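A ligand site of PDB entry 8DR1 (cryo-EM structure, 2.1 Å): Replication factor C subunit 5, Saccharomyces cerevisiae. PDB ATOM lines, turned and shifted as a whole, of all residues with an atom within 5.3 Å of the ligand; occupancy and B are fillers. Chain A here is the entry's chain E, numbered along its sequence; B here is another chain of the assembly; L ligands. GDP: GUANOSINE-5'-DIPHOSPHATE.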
ATOM      1  N   VAL A   5     -24.593 -14.893  25.588  1.00  0.00           N
ATOM      2  CA  VAL A   5     -24.319 -14.858  24.151  1.00  0.00           C
ATOM      3  C   VAL A   5     -25.598 -15.025  23.355  1.00  0.00           C
ATOM      4  O   VAL A   5     -25.719 -14.501  22.240  1.00  0.00           O
ATOM      5  CB  VAL A   5     -23.272 -15.927  23.790  1.00  0.00           C
ATOM      6  CG1 VAL A   5     -23.860 -17.323  23.915  1.00  0.00           C
ATOM      7  CG2 VAL A   5     -22.754 -15.693  22.376  1.00  0.00           C
ATOM      8  N   ASP A   6     -26.579 -15.750  23.898  1.00  0.00           N
ATOM      9  CA  ASP A   6     -27.838 -15.982  23.195  1.00  0.00           C
ATOM     10  C   ASP A   6     -28.915 -14.979  23.582  1.00  0.00           C
ATOM     11  O   ASP A   6     -29.709 -14.565  22.737  1.00  0.00           O
ATOM     12  CB  ASP A   6     -28.335 -17.406  23.486  1.00  0.00           C
ATOM     13  CG  ASP A   6     -27.442 -18.465  22.877  1.00  0.00           C
ATOM     14  OD1 ASP A   6     -26.978 -18.283  21.732  1.00  0.00           O
ATOM     15  OD2 ASP A   6     -27.201 -19.498  23.553  1.00  0.00           O
ATOM     16  N   TYR A   8     -28.877 -11.846  24.324  1.00  0.00           N
ATOM     17  CA  TYR A   8     -28.758 -10.493  23.773  1.00  0.00           C
ATOM     18  C   TYR A   8     -28.391 -10.496  22.294  1.00  0.00           C
ATOM     19  O   TYR A   8     -27.880  -9.501  21.779  1.00  0.00           O
ATOM     20  CB  TYR A   8     -27.710  -9.703  24.558  1.00  0.00           C
ATOM     21  CG  TYR A   8     -28.063  -9.540  26.023  1.00  0.00           C
ATOM     22  CD1 TYR A   8     -29.100  -8.698  26.421  1.00  0.00           C
ATOM     23  CD2 TYR A   8     -27.351 -10.214  27.004  1.00  0.00           C
ATOM     24  CE1 TYR A   8     -29.426  -8.550  27.758  1.00  0.00           C
ATOM     25  CE2 TYR A   8     -27.668 -10.068  28.344  1.00  0.00           C
ATOM     26  CZ  TYR A   8     -28.707  -9.235  28.711  1.00  0.00           C
ATOM     27  OH  TYR A   8     -29.019  -9.079  30.042  1.00  0.00           O
ATOM     28  N   ARG A   9     -28.655 -11.594  21.580  1.00  0.00           N
ATOM     29  CA  ARG A   9     -28.365 -11.634  20.152  1.00  0.00           C
ATOM     30  C   ARG A   9     -29.342 -10.728  19.401  1.00  0.00           C
ATOM     31  O   ARG A   9     -30.557 -10.859  19.587  1.00  0.00           O
ATOM     32  CB  ARG A   9     -28.459 -13.059  19.613  1.00  0.00           C
ATOM     33  CG  ARG A   9     -28.311 -13.143  18.102  1.00  0.00           C
ATOM     34  CD  ARG A   9     -27.962 -14.549  17.626  1.00  0.00           C
ATOM     35  NE  ARG A   9     -28.933 -15.540  18.082  1.00  0.00           N
ATOM     36  CZ  ARG A   9     -28.729 -16.404  19.073  1.00  0.00           C
ATOM     37  NH1 ARG A   9     -27.585 -16.436  19.744  1.00  0.00           N
ATOM     38  NH2 ARG A   9     -29.688 -17.265  19.400  1.00  0.00           N
ATOM     39  N   PRO A  10     -28.870  -9.806  18.564  1.00  0.00           N
ATOM     40  CA  PRO A  10     -29.796  -8.940  17.831  1.00  0.00           C
ATOM     41  C   PRO A  10     -30.723  -9.742  16.927  1.00  0.00           C
ATOM     42  O   PRO A  10     -30.358 -10.795  16.406  1.00  0.00           O
ATOM     43  CB  PRO A  10     -28.860  -8.034  17.002  1.00  0.00           C
ATOM     44  CG  PRO A  10     -27.529  -8.130  17.651  1.00  0.00           C
ATOM     45  CD  PRO A  10     -27.456  -9.478  18.271  1.00  0.00           C
ATOM     46  N   ALA A  15     -30.659  -3.523  14.761  1.00  0.00           N
ATOM     47  CA  ALA A  15     -30.076  -3.858  16.040  1.00  0.00           C
ATOM     48  C   ALA A  15     -28.611  -4.293  15.942  1.00  0.00           C
ATOM     49  O   ALA A  15     -27.976  -4.485  16.977  1.00  0.00           O
ATOM     50  CB  ALA A  15     -30.885  -4.971  16.720  1.00  0.00           C
ATOM     51  N   LEU A  16     -28.083  -4.459  14.730  1.00  0.00           N
ATOM     52  CA  LEU A  16     -26.687  -4.840  14.576  1.00  0.00           C
ATOM     53  C   LEU A  16     -25.781  -3.738  15.122  1.00  0.00           C
ATOM     54  O   LEU A  16     -26.075  -2.554  14.997  1.00  0.00           O
ATOM     55  CB  LEU A  16     -26.376  -5.127  13.105  1.00  0.00           C
ATOM     56  CG  LEU A  16     -27.148  -6.284  12.478  1.00  0.00           C
ATOM     57  CD1 LEU A  16     -26.803  -6.435  11.011  1.00  0.00           C
ATOM     58  CD2 LEU A  16     -26.887  -7.596  13.229  1.00  0.00           C
ATOM     59  N   SER A  17     -24.652  -4.153  15.715  1.00  0.00           N
ATOM     60  CA  SER A  17     -23.807  -3.245  16.472  1.00  0.00           C
ATOM     61  C   SER A  17     -22.398  -3.088  15.926  1.00  0.00           C
ATOM     62  O   SER A  17     -21.603  -2.362  16.531  1.00  0.00           O
ATOM     63  CB  SER A  17     -23.721  -3.712  17.929  1.00  0.00           C
ATOM     64  OG  SER A  17     -25.008  -3.953  18.476  1.00  0.00           O
ATOM     65  N   HIS A  18     -22.055  -3.738  14.809  1.00  0.00           N
ATOM     66  CA  HIS A  18     -20.725  -3.577  14.248  1.00  0.00           C
ATOM     67  C   HIS A  18     -20.777  -3.766  12.733  1.00  0.00           C
ATOM     68  O   HIS A  18     -21.720  -4.362  12.201  1.00  0.00           O
ATOM     69  CB  HIS A  18     -19.712  -4.550  14.878  1.00  0.00           C
ATOM     70  CG  HIS A  18     -19.997  -5.991  14.596  1.00  0.00           C
ATOM     71  ND1 HIS A  18     -19.508  -6.649  13.483  1.00  0.00           N
ATOM     72  CD2 HIS A  18     -20.711  -6.919  15.285  1.00  0.00           C
ATOM     73  CE1 HIS A  18     -19.908  -7.907  13.501  1.00  0.00           C
ATOM     74  NE2 HIS A  18     -20.641  -8.089  14.584  1.00  0.00           N
ATOM     75  N   PRO A  44     -14.611 -14.838   8.971  1.00  0.00           N
ATOM     76  CA  PRO A  44     -14.096 -15.568  10.135  1.00  0.00           C
ATOM     77  C   PRO A  44     -15.230 -16.092  11.007  1.00  0.00           C
ATOM     78  O   PRO A  44     -16.313 -15.504  11.100  1.00  0.00           O
ATOM     79  CB  PRO A  44     -13.256 -14.526  10.883  1.00  0.00           C
ATOM     80  CG  PRO A  44     -12.938 -13.483   9.866  1.00  0.00           C
ATOM     81  CD  PRO A  44     -14.092 -13.460   8.920  1.00  0.00           C
ATOM     82  N   ASN A  45     -14.968 -17.231  11.654  1.00  0.00           N
ATOM     83  CA  ASN A  45     -15.981 -17.879  12.476  1.00  0.00           C
ATOM     84  C   ASN A  45     -16.336 -17.023  13.682  1.00  0.00           C
ATOM     85  O   ASN A  45     -15.490 -16.348  14.264  1.00  0.00           O
ATOM     86  CB  ASN A  45     -15.474 -19.256  12.918  1.00  0.00           C
ATOM     87  CG  ASN A  45     -16.351 -19.890  13.991  1.00  0.00           C
ATOM     88  OD1 ASN A  45     -16.422 -19.402  15.127  1.00  0.00           O
ATOM     89  ND2 ASN A  45     -17.028 -20.973  13.641  1.00  0.00           N
ATOM     90  N   GLY A  46     -17.618 -17.071  14.063  1.00  0.00           N
ATOM     91  CA  GLY A  46     -18.062 -16.402  15.272  1.00  0.00           C
ATOM     92  C   GLY A  46     -18.167 -14.897  15.179  1.00  0.00           C
ATOM     93  O   GLY A  46     -18.123 -14.217  16.203  1.00  0.00           O
ATOM     94  N   THR A  47     -18.306 -14.339  13.973  1.00  0.00           N
ATOM     95  CA  THR A  47     -18.373 -12.902  13.789  1.00  0.00           C
ATOM     96  C   THR A  47     -19.804 -12.372  13.736  1.00  0.00           C
ATOM     97  O   THR A  47     -20.016 -11.184  14.025  1.00  0.00           O
ATOM     98  CB  THR A  47     -17.649 -12.484  12.502  1.00  0.00           C
ATOM     99  OG1 THR A  47     -18.209 -13.180  11.381  1.00  0.00           O
ATOM    100  CG2 THR A  47     -16.172 -12.789  12.610  1.00  0.00           C
ATOM    101  N   GLY A  48     -20.785 -13.205  13.383  1.00  0.00           N
ATOM    102  CA  GLY A  48     -22.159 -12.746  13.278  1.00  0.00           C
ATOM    103  C   GLY A  48     -22.778 -13.014  11.926  1.00  0.00           C
ATOM    104  O   GLY A  48     -23.724 -12.318  11.522  1.00  0.00           O
ATOM    105  N   LYS A  49     -22.270 -14.022  11.217  1.00  0.00           N
ATOM    106  CA  LYS A  49     -22.795 -14.317   9.885  1.00  0.00           C
ATOM    107  C   LYS A  49     -24.229 -14.844   9.962  1.00  0.00           C
ATOM    108  O   LYS A  49     -25.113 -14.373   9.232  1.00  0.00           O
ATOM    109  CB  LYS A  49     -21.885 -15.328   9.185  1.00  0.00           C
ATOM    110  CG  LYS A  49     -20.510 -14.789   8.837  1.00  0.00           C
ATOM    111  CD  LYS A  49     -19.725 -15.746   7.959  1.00  0.00           C
ATOM    112  CE  LYS A  49     -19.439 -17.063   8.665  1.00  0.00           C
ATOM    113  NZ  LYS A  49     -18.771 -16.875   9.983  1.00  0.00           N
ATOM    114  N   LYS A  50     -24.478 -15.828  10.830  1.00  0.00           N
ATOM    115  CA  LYS A  50     -25.826 -16.361  10.965  1.00  0.00           C
ATOM    116  C   LYS A  50     -26.786 -15.309  11.512  1.00  0.00           C
ATOM    117  O   LYS A  50     -27.952 -15.244  11.094  1.00  0.00           O
ATOM    118  CB  LYS A  50     -25.812 -17.597  11.866  1.00  0.00           C
ATOM    119  CG  LYS A  50     -27.076 -18.440  11.792  1.00  0.00           C
ATOM    120  CD  LYS A  50     -27.294 -19.016  10.404  1.00  0.00           C
ATOM    121  CE  LYS A  50     -28.309 -20.139  10.423  1.00  0.00           C
ATOM    122  NZ  LYS A  50     -29.686 -19.640  10.650  1.00  0.00           N
ATOM    123  N   THR A  51     -26.306 -14.475  12.433  1.00  0.00           N
ATOM    124  CA  THR A  51     -27.141 -13.386  12.942  1.00  0.00           C
ATOM    125  C   THR A  51     -27.567 -12.460  11.816  1.00  0.00           C
ATOM    126  O   THR A  51     -28.735 -12.059  11.736  1.00  0.00           O
ATOM    127  CB  THR A  51     -26.384 -12.615  14.026  1.00  0.00           C
ATOM    128  OG1 THR A  51     -25.877 -13.525  15.009  1.00  0.00           O
ATOM    129  CG2 THR A  51     -27.293 -11.593  14.695  1.00  0.00           C
ATOM    130  N   ARG A  52     -26.631 -12.122  10.924  1.00  0.00           N
ATOM    131  CA  ARG A  52     -26.963 -11.223   9.818  1.00  0.00           C
ATOM    132  C   ARG A  52     -27.885 -11.903   8.804  1.00  0.00           C
ATOM    133  O   ARG A  52     -28.766 -11.260   8.234  1.00  0.00           O
ATOM    134  CB  ARG A  52     -25.687 -10.736   9.149  1.00  0.00           C
ATOM    135  CG  ARG A  52     -25.188  -9.417   9.724  1.00  0.00           C
ATOM    136  CD  ARG A  52     -23.674  -9.342   9.770  1.00  0.00           C
ATOM    137  NE  ARG A  52     -23.218  -8.229  10.595  1.00  0.00           N
ATOM    138  CZ  ARG A  52     -23.216  -8.233  11.917  1.00  0.00           C
ATOM    139  NH1 ARG A  52     -23.603  -9.292  12.610  1.00  0.00           N
ATOM    140  NH2 ARG A  52     -22.806  -7.142  12.572  1.00  0.00           N
ATOM    141  N   VAL A 170     -23.686 -20.206   4.008  1.00  0.00           N
ATOM    142  CA  VAL A 170     -22.827 -19.566   4.994  1.00  0.00           C
ATOM    143  C   VAL A 170     -21.603 -20.444   5.191  1.00  0.00           C
ATOM    144  O   VAL A 170     -21.739 -21.651   5.445  1.00  0.00           O
ATOM    145  CB  VAL A 170     -23.554 -19.343   6.329  1.00  0.00           C
ATOM    146  CG1 VAL A 170     -22.682 -18.531   7.278  1.00  0.00           C
ATOM    147  CG2 VAL A 170     -24.888 -18.657   6.098  1.00  0.00           C
ATOM    148  N   ILE A 201     -19.911  -4.018  23.069  1.00  0.00           N
ATOM    149  CA  ILE A 201     -20.933  -5.049  23.228  1.00  0.00           C
ATOM    150  C   ILE A 201     -20.824  -5.684  24.618  1.00  0.00           C
ATOM    151  O   ILE A 201     -21.832  -5.905  25.303  1.00  0.00           O
ATOM    152  CB  ILE A 201     -20.802  -6.098  22.110  1.00  0.00           C
ATOM    153  CG1 ILE A 201     -21.182  -5.474  20.763  1.00  0.00           C
ATOM    154  CG2 ILE A 201     -21.669  -7.310  22.411  1.00  0.00           C
ATOM    155  CD1 ILE A 201     -20.863  -6.343  19.557  1.00  0.00           C
ATOM    156  N   LEU A 230     -16.476 -12.942  18.364  1.00  0.00           N
ATOM    157  CA  LEU A 230     -17.411 -12.314  19.287  1.00  0.00           C
ATOM    158  C   LEU A 230     -18.101 -13.337  20.177  1.00  0.00           C
ATOM    159  O   LEU A 230     -18.291 -13.102  21.374  1.00  0.00           O
ATOM    160  CB  LEU A 230     -18.445 -11.499  18.492  1.00  0.00           C
ATOM    161  CG  LEU A 230     -19.484 -10.708  19.301  1.00  0.00           C
ATOM    162  CD1 LEU A 230     -18.820  -9.868  20.383  1.00  0.00           C
ATOM    163  CD2 LEU A 230     -20.302  -9.831  18.370  1.00  0.00           C
ATOM    164  N   ARG A 231     -18.507 -14.481  19.611  1.00  0.00           N
ATOM    165  CA  ARG A 231     -19.154 -15.512  20.400  1.00  0.00           C
ATOM    166  C   ARG A 231     -18.234 -15.992  21.508  1.00  0.00           C
ATOM    167  O   ARG A 231     -18.644 -16.142  22.668  1.00  0.00           O
ATOM    168  CB  ARG A 231     -19.564 -16.684  19.498  1.00  0.00           C
ATOM    169  CG  ARG A 231     -19.969 -17.944  20.259  1.00  0.00           C
ATOM    170  CD  ARG A 231     -20.585 -18.996  19.339  1.00  0.00           C
ATOM    171  NE  ARG A 231     -19.636 -19.495  18.350  1.00  0.00           N
ATOM    172  CZ  ARG A 231     -19.708 -19.275  17.037  1.00  0.00           C
ATOM    173  NH1 ARG A 231     -20.683 -18.553  16.507  1.00  0.00           N
ATOM    174  NH2 ARG A 231     -18.783 -19.800  16.241  1.00  0.00           N
ATOM    175  N   LEU A 234     -18.031 -13.322  24.297  1.00  0.00           N
ATOM    176  CA  LEU A 234     -19.177 -13.304  25.189  1.00  0.00           C
ATOM    177  C   LEU A 234     -19.179 -14.507  26.124  1.00  0.00           C
ATOM    178  O   LEU A 234     -19.426 -14.373  27.340  1.00  0.00           O
ATOM    179  CB  LEU A 234     -20.478 -13.254  24.384  1.00  0.00           C
ATOM    180  CG  LEU A 234     -20.763 -11.917  23.688  1.00  0.00           C
ATOM    181  CD1 LEU A 234     -21.607 -12.123  22.442  1.00  0.00           C
ATOM    182  CD2 LEU A 234     -21.435 -10.951  24.653  1.00  0.00           C
ATOM    183  N   SER B 695     -26.815 -20.227  18.492  1.00  0.00           N
ATOM    184  CA  SER B 695     -26.470 -19.788  17.139  1.00  0.00           C
ATOM    185  C   SER B 695     -25.043 -20.256  16.873  1.00  0.00           C
ATOM    186  O   SER B 695     -24.081 -19.541  17.184  1.00  0.00           O
ATOM    187  CB  SER B 695     -26.610 -18.277  16.992  1.00  0.00           C
ATOM    188  OG  SER B 695     -26.271 -17.858  15.679  1.00  0.00           O
ATOM    189  N   THR B 696     -24.900 -21.441  16.301  1.00  0.00           N
ATOM    190  CA  THR B 696     -23.592 -22.029  16.036  1.00  0.00           C
ATOM    191  C   THR B 696     -23.818 -23.378  15.358  1.00  0.00           C
ATOM    192  O   THR B 696     -24.947 -23.870  15.266  1.00  0.00           O
ATOM    193  CB  THR B 696     -22.763 -22.207  17.309  1.00  0.00           C
ATOM    194  OG1 THR B 696     -21.547 -22.889  17.010  1.00  0.00           O
ATOM    195  CG2 THR B 696     -23.545 -23.010  18.348  1.00  0.00           C
ATOM    196  N   TYR B 705     -19.380 -23.382  23.476  1.00  0.00           N
ATOM    197  CA  TYR B 705     -20.502 -23.380  24.417  1.00  0.00           C
ATOM    198  C   TYR B 705     -20.264 -24.333  25.581  1.00  0.00           C
ATOM    199  O   TYR B 705     -20.614 -24.017  26.724  1.00  0.00           O
ATOM    200  CB  TYR B 705     -21.790 -23.769  23.682  1.00  0.00           C
ATOM    201  CG  TYR B 705     -22.508 -22.606  23.040  1.00  0.00           C
ATOM    202  CD1 TYR B 705     -23.405 -21.821  23.767  1.00  0.00           C
ATOM    203  CD2 TYR B 705     -22.307 -22.284  21.701  1.00  0.00           C
ATOM    204  CE1 TYR B 705     -24.069 -20.771  23.189  1.00  0.00           C
ATOM    205  CE2 TYR B 705     -22.978 -21.232  21.110  1.00  0.00           C
ATOM    206  CZ  TYR B 705     -23.853 -20.471  21.856  1.00  0.00           C
ATOM    207  OH  TYR B 705     -24.514 -19.421  21.269  1.00  0.00           O
HETATM  208  PB  GDP L   1     -21.077 -16.862  12.895  1.00  0.00           P
HETATM  209  O1B GDP L   1     -20.401 -15.826  12.021  1.00  0.00           O
HETATM  210  O2B GDP L   1     -22.367 -17.302  12.236  1.00  0.00           O
HETATM  211  O3B GDP L   1     -20.162 -18.050  13.076  1.00  0.00           O
HETATM  212  O3A GDP L   1     -21.401 -16.196  14.362  1.00  0.00           O
HETATM  213  PA  GDP L   1     -22.908 -15.836  14.913  1.00  0.00           P
HETATM  214  O1A GDP L   1     -23.755 -15.259  13.801  1.00  0.00           O
HETATM  215  O2A GDP L   1     -23.568 -17.088  15.448  1.00  0.00           O
HETATM  216  O5' GDP L   1     -22.765 -14.727  16.113  1.00  0.00           O
HETATM  217  C5' GDP L   1     -22.209 -15.139  17.335  1.00  0.00           C
HETATM  218  C4' GDP L   1     -22.751 -14.299  18.484  1.00  0.00           C
HETATM  219  O4' GDP L   1     -22.147 -12.804  18.370  1.00  0.00           O
HETATM  220  C3' GDP L   1     -24.049 -14.200  18.433  1.00  0.00           C
HETATM  221  O3' GDP L   1     -24.661 -15.208  19.357  1.00  0.00           O
HETATM  222  C2' GDP L   1     -24.375 -12.778  18.914  1.00  0.00           C
HETATM  223  O2' GDP L   1     -24.693 -12.794  20.232  1.00  0.00           O
HETATM  224  C1' GDP L   1     -23.088 -11.959  18.703  1.00  0.00           C
HETATM  225  N9  GDP L   1     -23.248 -10.970  17.613  1.00  0.00           N
HETATM  226  C8  GDP L   1     -23.023 -11.110  16.297  1.00  0.00           C
HETATM  227  N7  GDP L   1     -23.300  -9.917  15.726  1.00  0.00           N
HETATM  228  C5  GDP L   1     -23.674  -9.078  16.686  1.00  0.00           C
HETATM  229  C6  GDP L   1     -24.098  -7.595  16.641  1.00  0.00           C
HETATM  230  O6  GDP L   1     -24.138  -7.025  15.601  1.00  0.00           O
HETATM  231  N1  GDP L   1     -24.454  -6.922  17.846  1.00  0.00           N
HETATM  232  C2  GDP L   1     -24.412  -7.625  19.103  1.00  0.00           C
HETATM  233  N2  GDP L   1     -24.774  -6.951  20.328  1.00  0.00           N
HETATM  234  N3  GDP L   1     -24.004  -9.034  19.139  1.00  0.00           N
HETATM  235  C4  GDP L   1     -23.634  -9.729  17.877  1.00  0.00           C
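N of Lys 49 is in hydrogen-bond range of O1B of the ligand.
The side-chain amino group (NZ) of Lys 49 lies within salt-bridge range of an oxygen (O1B) of the ligand, at 2.8 Å.
O2A of the ligand sits close to O of Ser 695 of chain B.
OG of Ser 695 of chain B sits at hydrogen-bond distance from O2A of the ligand, 2.8 Å away.
O of Val 5 is in hydrogen-bond range of O2' of the ligand.
An oxygen (O3B) of the ligand sits at hydrogen-bond distance from the backbone NH of Gly 46 (2.9 Å).
The backbone NH (N) of Ser 17 sits at hydrogen-bond distance from an oxygen (O6) of the ligand (2.9 Å).
The side-chain hydroxyl (OG) of Ser 17 is in hydrogen-bond range of a nitrogen (N1) of the ligand.
N of Lys 50 sits at hydrogen-bond distance from O2B of the ligand.
The backbone NH of Gly 48 sits at hydrogen-bond distance from an oxygen (O1B) of the ligand (3.0 Å).
The backbone NH of Thr 51 sits at hydrogen-bond distance from an oxygen (O1A) of the ligand (3.0 Å).
An oxygen (O1A) of the ligand lies within hydrogen-bond range of the side-chain hydroxyl of Thr 51, at 3.0 Å.
A nitrogen (N7) of the ligand is in hydrogen-bond range of the guanidinium group (NH1) of Arg 52, 3.2 Å away.
The guanidinium group of Arg 9 sits at hydrogen-bond distance from an oxygen (O3') of the ligand.
The backbone NH of Thr 47 is in hydrogen-bond range of an oxygen (O1B) of the ligand, 3.2 Å away.
The side-chain hydroxyl (OG1) of Thr 47 lies within hydrogen-bond range of an oxygen (O1B) of the ligand, 3.5 Å away.
NH1 of Arg 231 lies within salt-bridge range of O2A of the ligand, 3.4 Å away.
A ring nitrogen (NE2) of His 18 is in hydrogen-bond range of a nitrogen (N7) of the ligand, 3.4 Å away.
N of Leu 230 sits at hydrogen-bond distance from O of Gly 46.
OG of Ser 17 sits at hydrogen-bond distance from O of Ala 15, at 3.4 Å.
O of Gly 48 lies within hydrogen-bond range of NH1 of Arg 52 (3.2 Å).
The backbone carbonyl oxygen (O) of His 18 sits at hydrogen-bond distance from the guanidinium group (NH2) of Arg 52 (3.0 Å).
The side-chain carboxylate (OD1) of Asp 6 lies within salt-bridge range of the guanidinium group (NH1) of Arg 9 (2.8 Å).
The backbone carbonyl oxygen of Thr 47 sits at hydrogen-bond distance from a ring nitrogen (NE2) of His 18 (3.2 Å).
The side-chain hydroxyl of Thr 47 lies within hydrogen-bond range of the backbone carbonyl oxygen of Pro 44, at 3.0 Å.
The side-chain amide oxygen of Asn 45 lies within hydrogen-bond range of the guanidinium group of Arg 231.
Merely in contact with the ligand: Leu 230 (3.2 Å), Pro 10 (3.3 Å), Leu 16 (3.5 Å), Ile 201 (3.8 Å) and Leu 234 (3.9 Å).
Hydrophobic or aromatic side chains that line the ligand: Val 5, Pro 10, Leu 16, His 18, Ile 201, Leu 230 and Leu 234.
The nearest printed residue that does not touch the ligand is Asn 45 (4.01 Å).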
